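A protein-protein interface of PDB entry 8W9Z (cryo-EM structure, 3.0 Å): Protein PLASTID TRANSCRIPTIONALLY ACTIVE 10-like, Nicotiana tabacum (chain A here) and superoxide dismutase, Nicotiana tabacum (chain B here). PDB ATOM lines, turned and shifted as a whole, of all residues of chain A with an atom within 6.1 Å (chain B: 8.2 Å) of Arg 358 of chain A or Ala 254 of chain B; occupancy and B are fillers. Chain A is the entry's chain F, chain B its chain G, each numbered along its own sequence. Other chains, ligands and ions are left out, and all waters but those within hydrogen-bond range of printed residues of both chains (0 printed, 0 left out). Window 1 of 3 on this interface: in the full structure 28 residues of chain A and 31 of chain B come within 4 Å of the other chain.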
ATOM      1  N   PRO A 306     -12.941 -15.350   7.997  1.00  0.00           N
ATOM      2  CA  PRO A 306     -12.483 -16.414   8.902  1.00  0.00           C
ATOM      3  C   PRO A 306     -10.982 -16.407   9.136  1.00  0.00           C
ATOM      4  O   PRO A 306     -10.200 -16.692   8.223  1.00  0.00           O
ATOM      5  CB  PRO A 306     -12.926 -17.696   8.183  1.00  0.00           C
ATOM      6  CG  PRO A 306     -13.978 -17.260   7.213  1.00  0.00           C
ATOM      7  CD  PRO A 306     -13.564 -15.892   6.781  1.00  0.00           C
ATOM      8  N   LYS A 308      -8.383 -17.996  12.145  1.00  0.00           N
ATOM      9  CA  LYS A 308      -8.388 -18.889  13.295  1.00  0.00           C
ATOM     10  C   LYS A 308      -7.473 -18.349  14.394  1.00  0.00           C
ATOM     11  O   LYS A 308      -7.028 -17.200  14.365  1.00  0.00           O
ATOM     12  CB  LYS A 308      -8.000 -20.300  12.863  1.00  0.00           C
ATOM     13  CG  LYS A 308      -9.051 -20.983  12.002  1.00  0.00           C
ATOM     14  CD  LYS A 308     -10.231 -21.455  12.830  1.00  0.00           C
ATOM     15  CE  LYS A 308      -9.848 -22.632  13.709  1.00  0.00           C
ATOM     16  NZ  LYS A 308     -11.016 -23.172  14.455  1.00  0.00           N
ATOM     17  N   ASP A 311      -3.142 -17.941  13.648  1.00  0.00           N
ATOM     18  CA  ASP A 311      -2.676 -17.002  12.633  1.00  0.00           C
ATOM     19  C   ASP A 311      -2.639 -15.567  13.140  1.00  0.00           C
ATOM     20  O   ASP A 311      -1.925 -14.734  12.566  1.00  0.00           O
ATOM     21  CB  ASP A 311      -3.564 -17.091  11.392  1.00  0.00           C
ATOM     22  CG  ASP A 311      -3.662 -18.501  10.847  1.00  0.00           C
ATOM     23  OD1 ASP A 311      -2.681 -19.262  10.981  1.00  0.00           O
ATOM     24  OD2 ASP A 311      -4.722 -18.849  10.284  1.00  0.00           O
ATOM     25  N   ARG A 345     -13.680 -12.197   2.013  1.00  0.00           N
ATOM     26  CA  ARG A 345     -12.229 -12.285   2.007  1.00  0.00           C
ATOM     27  C   ARG A 345     -11.645 -10.892   1.812  1.00  0.00           C
ATOM     28  O   ARG A 345     -12.311  -9.983   1.312  1.00  0.00           O
ATOM     29  CB  ARG A 345     -11.721 -13.228   0.908  1.00  0.00           C
ATOM     30  CG  ARG A 345     -12.101 -12.798  -0.498  1.00  0.00           C
ATOM     31  CD  ARG A 345     -11.529 -13.745  -1.539  1.00  0.00           C
ATOM     32  NE  ARG A 345     -10.071 -13.787  -1.497  1.00  0.00           N
ATOM     33  CZ  ARG A 345      -9.281 -12.975  -2.189  1.00  0.00           C
ATOM     34  NH1 ARG A 345      -9.806 -12.051  -2.980  1.00  0.00           N
ATOM     35  NH2 ARG A 345      -7.963 -13.085  -2.089  1.00  0.00           N
ATOM     36  N   ASP A 352      -3.488 -13.667   2.219  1.00  0.00           N
ATOM     37  CA  ASP A 352      -3.736 -15.059   1.864  1.00  0.00           C
ATOM     38  C   ASP A 352      -2.540 -15.968   2.119  1.00  0.00           C
ATOM     39  O   ASP A 352      -2.683 -17.190   2.010  1.00  0.00           O
ATOM     40  CB  ASP A 352      -4.150 -15.158   0.394  1.00  0.00           C
ATOM     41  CG  ASP A 352      -3.052 -14.716  -0.551  1.00  0.00           C
ATOM     42  OD1 ASP A 352      -2.224 -13.872  -0.148  1.00  0.00           O
ATOM     43  OD2 ASP A 352      -3.015 -15.213  -1.696  1.00  0.00           O
ATOM     44  N   ILE A 355      -2.850 -17.466   6.318  1.00  0.00           N
ATOM     45  CA  ILE A 355      -3.988 -18.233   6.811  1.00  0.00           C
ATOM     46  C   ILE A 355      -3.724 -19.701   6.509  1.00  0.00           C
ATOM     47  O   ILE A 355      -3.738 -20.119   5.347  1.00  0.00           O
ATOM     48  CB  ILE A 355      -5.305 -17.759   6.183  1.00  0.00           C
ATOM     49  CG1 ILE A 355      -5.569 -16.295   6.536  1.00  0.00           C
ATOM     50  CG2 ILE A 355      -6.458 -18.636   6.644  1.00  0.00           C
ATOM     51  CD1 ILE A 355      -6.840 -15.744   5.935  1.00  0.00           C
ATOM     52  N   PHE A 356      -3.484 -20.488   7.556  1.00  0.00           N
ATOM     53  CA  PHE A 356      -3.252 -21.920   7.418  1.00  0.00           C
ATOM     54  C   PHE A 356      -4.359 -22.772   8.014  1.00  0.00           C
ATOM     55  O   PHE A 356      -4.625 -23.861   7.501  1.00  0.00           O
ATOM     56  CB  PHE A 356      -1.920 -22.309   8.072  1.00  0.00           C
ATOM     57  CG  PHE A 356      -0.730 -21.609   7.483  1.00  0.00           C
ATOM     58  CD1 PHE A 356      -0.082 -22.129   6.377  1.00  0.00           C
ATOM     59  CD2 PHE A 356      -0.259 -20.430   8.035  1.00  0.00           C
ATOM     60  CE1 PHE A 356       1.011 -21.488   5.833  1.00  0.00           C
ATOM     61  CE2 PHE A 356       0.835 -19.784   7.495  1.00  0.00           C
ATOM     62  CZ  PHE A 356       1.471 -20.314   6.392  1.00  0.00           C
ATOM     63  N   ASN A 357      -5.006 -22.308   9.077  1.00  0.00           N
ATOM     64  CA  ASN A 357      -6.144 -22.995   9.672  1.00  0.00           C
ATOM     65  C   ASN A 357      -7.427 -22.383   9.125  1.00  0.00           C
ATOM     66  O   ASN A 357      -7.600 -21.160   9.161  1.00  0.00           O
ATOM     67  CB  ASN A 357      -6.111 -22.890  11.196  1.00  0.00           C
ATOM     68  CG  ASN A 357      -4.787 -23.332  11.782  1.00  0.00           C
ATOM     69  OD1 ASN A 357      -4.110 -24.202  11.233  1.00  0.00           O
ATOM     70  ND2 ASN A 357      -4.407 -22.731  12.904  1.00  0.00           N
ATOM     71  N   ARG A 358      -8.316 -23.229   8.610  1.00  0.00           N
ATOM     72  CA  ARG A 358      -9.528 -22.768   7.953  1.00  0.00           C
ATOM     73  C   ARG A 358     -10.733 -23.547   8.458  1.00  0.00           C
ATOM     74  O   ARG A 358     -10.612 -24.668   8.959  1.00  0.00           O
ATOM     75  CB  ARG A 358      -9.420 -22.897   6.428  1.00  0.00           C
ATOM     76  CG  ARG A 358      -8.267 -22.113   5.831  1.00  0.00           C
ATOM     77  CD  ARG A 358      -8.253 -22.203   4.321  1.00  0.00           C
ATOM     78  NE  ARG A 358      -7.139 -21.456   3.747  1.00  0.00           N
ATOM     79  CZ  ARG A 358      -7.182 -20.159   3.460  1.00  0.00           C
ATOM     80  NH1 ARG A 358      -8.286 -19.463   3.694  1.00  0.00           N
ATOM     81  NH2 ARG A 358      -6.122 -19.557   2.940  1.00  0.00           N
ATOM     82  N   PHE A 359     -11.905 -22.932   8.320  1.00  0.00           N
ATOM     83  CA  PHE A 359     -13.153 -23.560   8.725  1.00  0.00           C
ATOM     84  C   PHE A 359     -13.620 -24.540   7.658  1.00  0.00           C
ATOM     85  O   PHE A 359     -13.651 -24.209   6.468  1.00  0.00           O
ATOM     86  CB  PHE A 359     -14.231 -22.502   8.968  1.00  0.00           C
ATOM     87  CG  PHE A 359     -14.037 -21.711  10.228  1.00  0.00           C
ATOM     88  CD1 PHE A 359     -13.270 -20.560  10.228  1.00  0.00           C
ATOM     89  CD2 PHE A 359     -14.629 -22.114  11.412  1.00  0.00           C
ATOM     90  CE1 PHE A 359     -13.094 -19.829  11.385  1.00  0.00           C
ATOM     91  CE2 PHE A 359     -14.456 -21.387  12.571  1.00  0.00           C
ATOM     92  CZ  PHE A 359     -13.687 -20.244  12.556  1.00  0.00           C
ATOM     93  N   ASP A 360     -13.980 -25.751   8.084  1.00  0.00           N
ATOM     94  CA  ASP A 360     -14.522 -26.731   7.150  1.00  0.00           C
ATOM     95  C   ASP A 360     -15.999 -26.477   6.871  1.00  0.00           C
ATOM     96  O   ASP A 360     -16.436 -26.544   5.717  1.00  0.00           O
ATOM     97  CB  ASP A 360     -14.311 -28.146   7.690  1.00  0.00           C
ATOM     98  CG  ASP A 360     -14.782 -28.301   9.123  1.00  0.00           C
ATOM     99  OD1 ASP A 360     -15.209 -27.293   9.724  1.00  0.00           O
ATOM    100  OD2 ASP A 360     -14.726 -29.433   9.649  1.00  0.00           O
ATOM    101  N   ARG B 186      -8.200 -29.862  -1.087  1.00  0.00           N
ATOM    102  CA  ARG B 186      -8.093 -28.893   0.000  1.00  0.00           C
ATOM    103  C   ARG B 186      -7.471 -29.518   1.243  1.00  0.00           C
ATOM    104  O   ARG B 186      -6.429 -29.061   1.728  1.00  0.00           O
ATOM    105  CB  ARG B 186      -9.471 -28.317   0.328  1.00  0.00           C
ATOM    106  CG  ARG B 186     -10.119 -27.540  -0.802  1.00  0.00           C
ATOM    107  CD  ARG B 186     -11.500 -27.060  -0.391  1.00  0.00           C
ATOM    108  NE  ARG B 186     -12.193 -26.364  -1.469  1.00  0.00           N
ATOM    109  CZ  ARG B 186     -12.230 -25.042  -1.602  1.00  0.00           C
ATOM    110  NH1 ARG B 186     -11.610 -24.269  -0.722  1.00  0.00           N
ATOM    111  NH2 ARG B 186     -12.888 -24.494  -2.613  1.00  0.00           N
ATOM    112  N   LYS B 189      -3.950 -30.822   0.432  1.00  0.00           N
ATOM    113  CA  LYS B 189      -3.014 -29.801  -0.042  1.00  0.00           C
ATOM    114  C   LYS B 189      -1.997 -30.398  -1.017  1.00  0.00           C
ATOM    115  O   LYS B 189      -0.782 -30.320  -0.825  1.00  0.00           O
ATOM    116  CB  LYS B 189      -2.317 -29.109   1.134  1.00  0.00           C
ATOM    117  CG  LYS B 189      -3.262 -28.385   2.076  1.00  0.00           C
ATOM    118  CD  LYS B 189      -2.510 -27.719   3.214  1.00  0.00           C
ATOM    119  CE  LYS B 189      -1.756 -28.740   4.049  1.00  0.00           C
ATOM    120  NZ  LYS B 189      -1.016 -28.103   5.172  1.00  0.00           N
ATOM    121  N   ARG B 248      -5.198 -20.030 -12.310  1.00  0.00           N
ATOM    122  CA  ARG B 248      -6.206 -20.672 -11.475  1.00  0.00           C
ATOM    123  C   ARG B 248      -5.611 -21.190 -10.172  1.00  0.00           C
ATOM    124  O   ARG B 248      -6.277 -21.149  -9.134  1.00  0.00           O
ATOM    125  CB  ARG B 248      -6.890 -21.800 -12.245  1.00  0.00           C
ATOM    126  CG  ARG B 248      -7.863 -21.305 -13.301  1.00  0.00           C
ATOM    127  CD  ARG B 248      -8.749 -22.424 -13.807  1.00  0.00           C
ATOM    128  NE  ARG B 248      -8.082 -23.258 -14.800  1.00  0.00           N
ATOM    129  CZ  ARG B 248      -8.275 -23.155 -16.110  1.00  0.00           C
ATOM    130  NH1 ARG B 248      -9.123 -22.254 -16.587  1.00  0.00           N
ATOM    131  NH2 ARG B 248      -7.626 -23.955 -16.944  1.00  0.00           N
ATOM    132  N   MET B 249      -4.360 -21.656 -10.193  1.00  0.00           N
ATOM    133  CA  MET B 249      -3.718 -22.060  -8.945  1.00  0.00           C
ATOM    134  C   MET B 249      -3.436 -20.853  -8.058  1.00  0.00           C
ATOM    135  O   MET B 249      -3.557 -20.935  -6.830  1.00  0.00           O
ATOM    136  CB  MET B 249      -2.428 -22.826  -9.232  1.00  0.00           C
ATOM    137  CG  MET B 249      -1.798 -23.435  -7.988  1.00  0.00           C
ATOM    138  SD  MET B 249      -0.295 -24.370  -8.327  1.00  0.00           S
ATOM    139  CE  MET B 249       0.818 -23.055  -8.811  1.00  0.00           C
ATOM    140  N   ALA B 250      -3.059 -19.724  -8.662  1.00  0.00           N
ATOM    141  CA  ALA B 250      -2.893 -18.495  -7.894  1.00  0.00           C
ATOM    142  C   ALA B 250      -4.205 -18.069  -7.252  1.00  0.00           C
ATOM    143  O   ALA B 250      -4.226 -17.610  -6.104  1.00  0.00           O
ATOM    144  CB  ALA B 250      -2.351 -17.383  -8.792  1.00  0.00           C
ATOM    145  N   ARG B 251      -5.312 -18.213  -7.981  1.00  0.00           N
ATOM    146  CA  ARG B 251      -6.621 -17.911  -7.408  1.00  0.00           C
ATOM    147  C   ARG B 251      -6.976 -18.887  -6.293  1.00  0.00           C
ATOM    148  O   ARG B 251      -7.569 -18.496  -5.281  1.00  0.00           O
ATOM    149  CB  ARG B 251      -7.685 -17.932  -8.504  1.00  0.00           C
ATOM    150  CG  ARG B 251      -9.108 -17.737  -8.005  1.00  0.00           C
ATOM    151  CD  ARG B 251      -9.299 -16.364  -7.390  1.00  0.00           C
ATOM    152  NE  ARG B 251     -10.672 -16.156  -6.940  1.00  0.00           N
ATOM    153  CZ  ARG B 251     -11.117 -15.027  -6.400  1.00  0.00           C
ATOM    154  NH1 ARG B 251     -12.383 -14.927  -6.018  1.00  0.00           N
ATOM    155  NH2 ARG B 251     -10.298 -13.997  -6.242  1.00  0.00           N
ATOM    156  N   ALA B 252      -6.615 -20.161  -6.457  1.00  0.00           N
ATOM    157  CA  ALA B 252      -6.936 -21.165  -5.450  1.00  0.00           C
ATOM    158  C   ALA B 252      -6.103 -20.990  -4.188  1.00  0.00           C
ATOM    159  O   ALA B 252      -6.541 -21.385  -3.102  1.00  0.00           O
ATOM    160  CB  ALA B 252      -6.728 -22.566  -6.021  1.00  0.00           C
ATOM    161  N   GLN B 253      -4.905 -20.412  -4.309  1.00  0.00           N
ATOM    162  CA  GLN B 253      -4.062 -20.201  -3.136  1.00  0.00           C
ATOM    163  C   GLN B 253      -4.717 -19.288  -2.106  1.00  0.00           C
ATOM    164  O   GLN B 253      -4.258 -19.238  -0.961  1.00  0.00           O
ATOM    165  CB  GLN B 253      -2.705 -19.635  -3.551  1.00  0.00           C
ATOM    166  CG  GLN B 253      -1.768 -20.667  -4.155  1.00  0.00           C
ATOM    167  CD  GLN B 253      -0.418 -20.088  -4.521  1.00  0.00           C
ATOM    168  OE1 GLN B 253       0.508 -20.817  -4.874  1.00  0.00           O
ATOM    169  NE2 GLN B 253      -0.298 -18.768  -4.440  1.00  0.00           N
ATOM    170  N   ALA B 254      -5.773 -18.567  -2.485  1.00  0.00           N
ATOM    171  CA  ALA B 254      -6.561 -17.808  -1.524  1.00  0.00           C
ATOM    172  C   ALA B 254      -7.521 -18.683  -0.731  1.00  0.00           C
ATOM    173  O   ALA B 254      -8.126 -18.197   0.231  1.00  0.00           O
ATOM    174  CB  ALA B 254      -7.344 -16.705  -2.238  1.00  0.00           C
ATOM    175  N   PHE B 255      -7.675 -19.951  -1.107  1.00  0.00           N
ATOM    176  CA  PHE B 255      -8.528 -20.891  -0.393  1.00  0.00           C
ATOM    177  C   PHE B 255      -7.778 -22.077   0.189  1.00  0.00           C
ATOM    178  O   PHE B 255      -8.259 -22.675   1.153  1.00  0.00           O
ATOM    179  CB  PHE B 255      -9.640 -21.417  -1.313  1.00  0.00           C
ATOM    180  CG  PHE B 255     -10.555 -20.349  -1.833  1.00  0.00           C
ATOM    181  CD1 PHE B 255     -11.555 -19.826  -1.033  1.00  0.00           C
ATOM    182  CD2 PHE B 255     -10.423 -19.875  -3.127  1.00  0.00           C
ATOM    183  CE1 PHE B 255     -12.401 -18.845  -1.510  1.00  0.00           C
ATOM    184  CE2 PHE B 255     -11.266 -18.894  -3.609  1.00  0.00           C
ATOM    185  CZ  PHE B 255     -12.256 -18.378  -2.800  1.00  0.00           C
ATOM    186  N   VAL B 256      -6.625 -22.438  -0.369  1.00  0.00           N
ATOM    187  CA  VAL B 256      -5.792 -23.515   0.153  1.00  0.00           C
ATOM    188  C   VAL B 256      -4.350 -23.025   0.158  1.00  0.00           C
ATOM    189  O   VAL B 256      -3.826 -22.613  -0.883  1.00  0.00           O
ATOM    190  CB  VAL B 256      -5.934 -24.808  -0.666  1.00  0.00           C
ATOM    191  CG1 VAL B 256      -5.977 -24.502  -2.156  1.00  0.00           C
ATOM    192  CG2 VAL B 256      -4.800 -25.768  -0.346  1.00  0.00           C
ATOM    193  N   ASN B 257      -3.715 -23.056   1.327  1.00  0.00           N
ATOM    194  CA  ASN B 257      -2.360 -22.543   1.486  1.00  0.00           C
ATOM    195  C   ASN B 257      -1.362 -23.668   1.243  1.00  0.00           C
ATOM    196  O   ASN B 257      -1.408 -24.704   1.914  1.00  0.00           O
ATOM    197  CB  ASN B 257      -2.172 -21.943   2.880  1.00  0.00           C
ATOM    198  CG  ASN B 257      -0.959 -21.036   2.966  1.00  0.00           C
ATOM    199  OD1 ASN B 257       0.056 -21.270   2.312  1.00  0.00           O
ATOM    200  ND2 ASN B 257      -1.061 -19.990   3.777  1.00  0.00           N
ATOM    201  N   LEU B 258      -0.462 -23.459   0.288  1.00  0.00           N
ATOM    202  CA  LEU B 258       0.577 -24.423  -0.066  1.00  0.00           C
ATOM    203  C   LEU B 258       1.914 -23.838   0.381  1.00  0.00           C
ATOM    204  O   LEU B 258       2.598 -23.155  -0.385  1.00  0.00           O
ATOM    205  CB  LEU B 258       0.563 -24.717  -1.563  1.00  0.00           C
ATOM    206  CG  LEU B 258      -0.769 -25.184  -2.148  1.00  0.00           C
ATOM    207  CD1 LEU B 258      -0.657 -25.365  -3.651  1.00  0.00           C
ATOM    208  CD2 LEU B 258      -1.223 -26.473  -1.483  1.00  0.00           C
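Arg 251 of chain B touches Arg 345 of chain A (NH2 to NH1, 3.8 Å). Arg 345 of chain A touches Ala 254 of chain B (NH2 to CB, 3.7 Å). Gln 253 of chain B touches Asp 352 of chain A. Asp 352 of chain A touches Asn 257 of chain B (O to ND2, 3.7 Å). Phe 356 of chain A touches Asn 257 of chain B. NH2 of Arg 358 of chain A touches O of Ala 254 of chain B (3.6 Å).
NE of Arg 358 of chain A is in hydrogen-bond range of O of Phe 255 of chain B, at 3.1 Å. The backbone carbonyl oxygen of Ile 355 of chain A lies within hydrogen-bond range of the side-chain amide nitrogen of Asn 257 of chain B (3.1 Å).
The side-chain carboxylate of Asp 311 of chain A sits at hydrogen-bond distance from the backbone NH of Phe 356 of chain A, 3.4 Å away. The guanidinium group of Arg 358 of chain A is in hydrogen-bond range of the backbone carbonyl oxygen of Ile 355 of chain A (3.4 Å).
Of chain B, only Ala 254 (3.6 Å) and Phe 255 (3.1 Å) come within 4 Å of Arg 358 of chain A. Printed residues of chain A within 4 Å of Ala 254 of chain B: Arg 345 (3.7 Å) and Arg 358 (3.6 Å). Printed residues of chain A within 4 Å of Arg 251 of chain B: Arg 345 (3.8 Å). Of the printed residues of chain B, Phe 356 of chain A touches Asn 257. The nearest residue of chain B that does not touch Arg 358 of chain A is Val 256 of chain B (4.3 Å). The nearest printed residue of chain A that does not touch Asn 257 of chain B is Arg 358 of chain A (4.5 Å).
Printed residues of chain B that touch a printed residue of chain A: Arg 251, Gln 253, Ala 254, Phe 255 and Asn 257. Hydrophobic or aromatic side chains of chain B within 4 Å of the printed part of chain A: Ala 254. Hydrophobic or aromatic side chains of chain A within 4 Å of the printed part of chain B: Phe 356. Along chain A the printed residues that touch a printed residue of chain B span positions 345 to 358.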
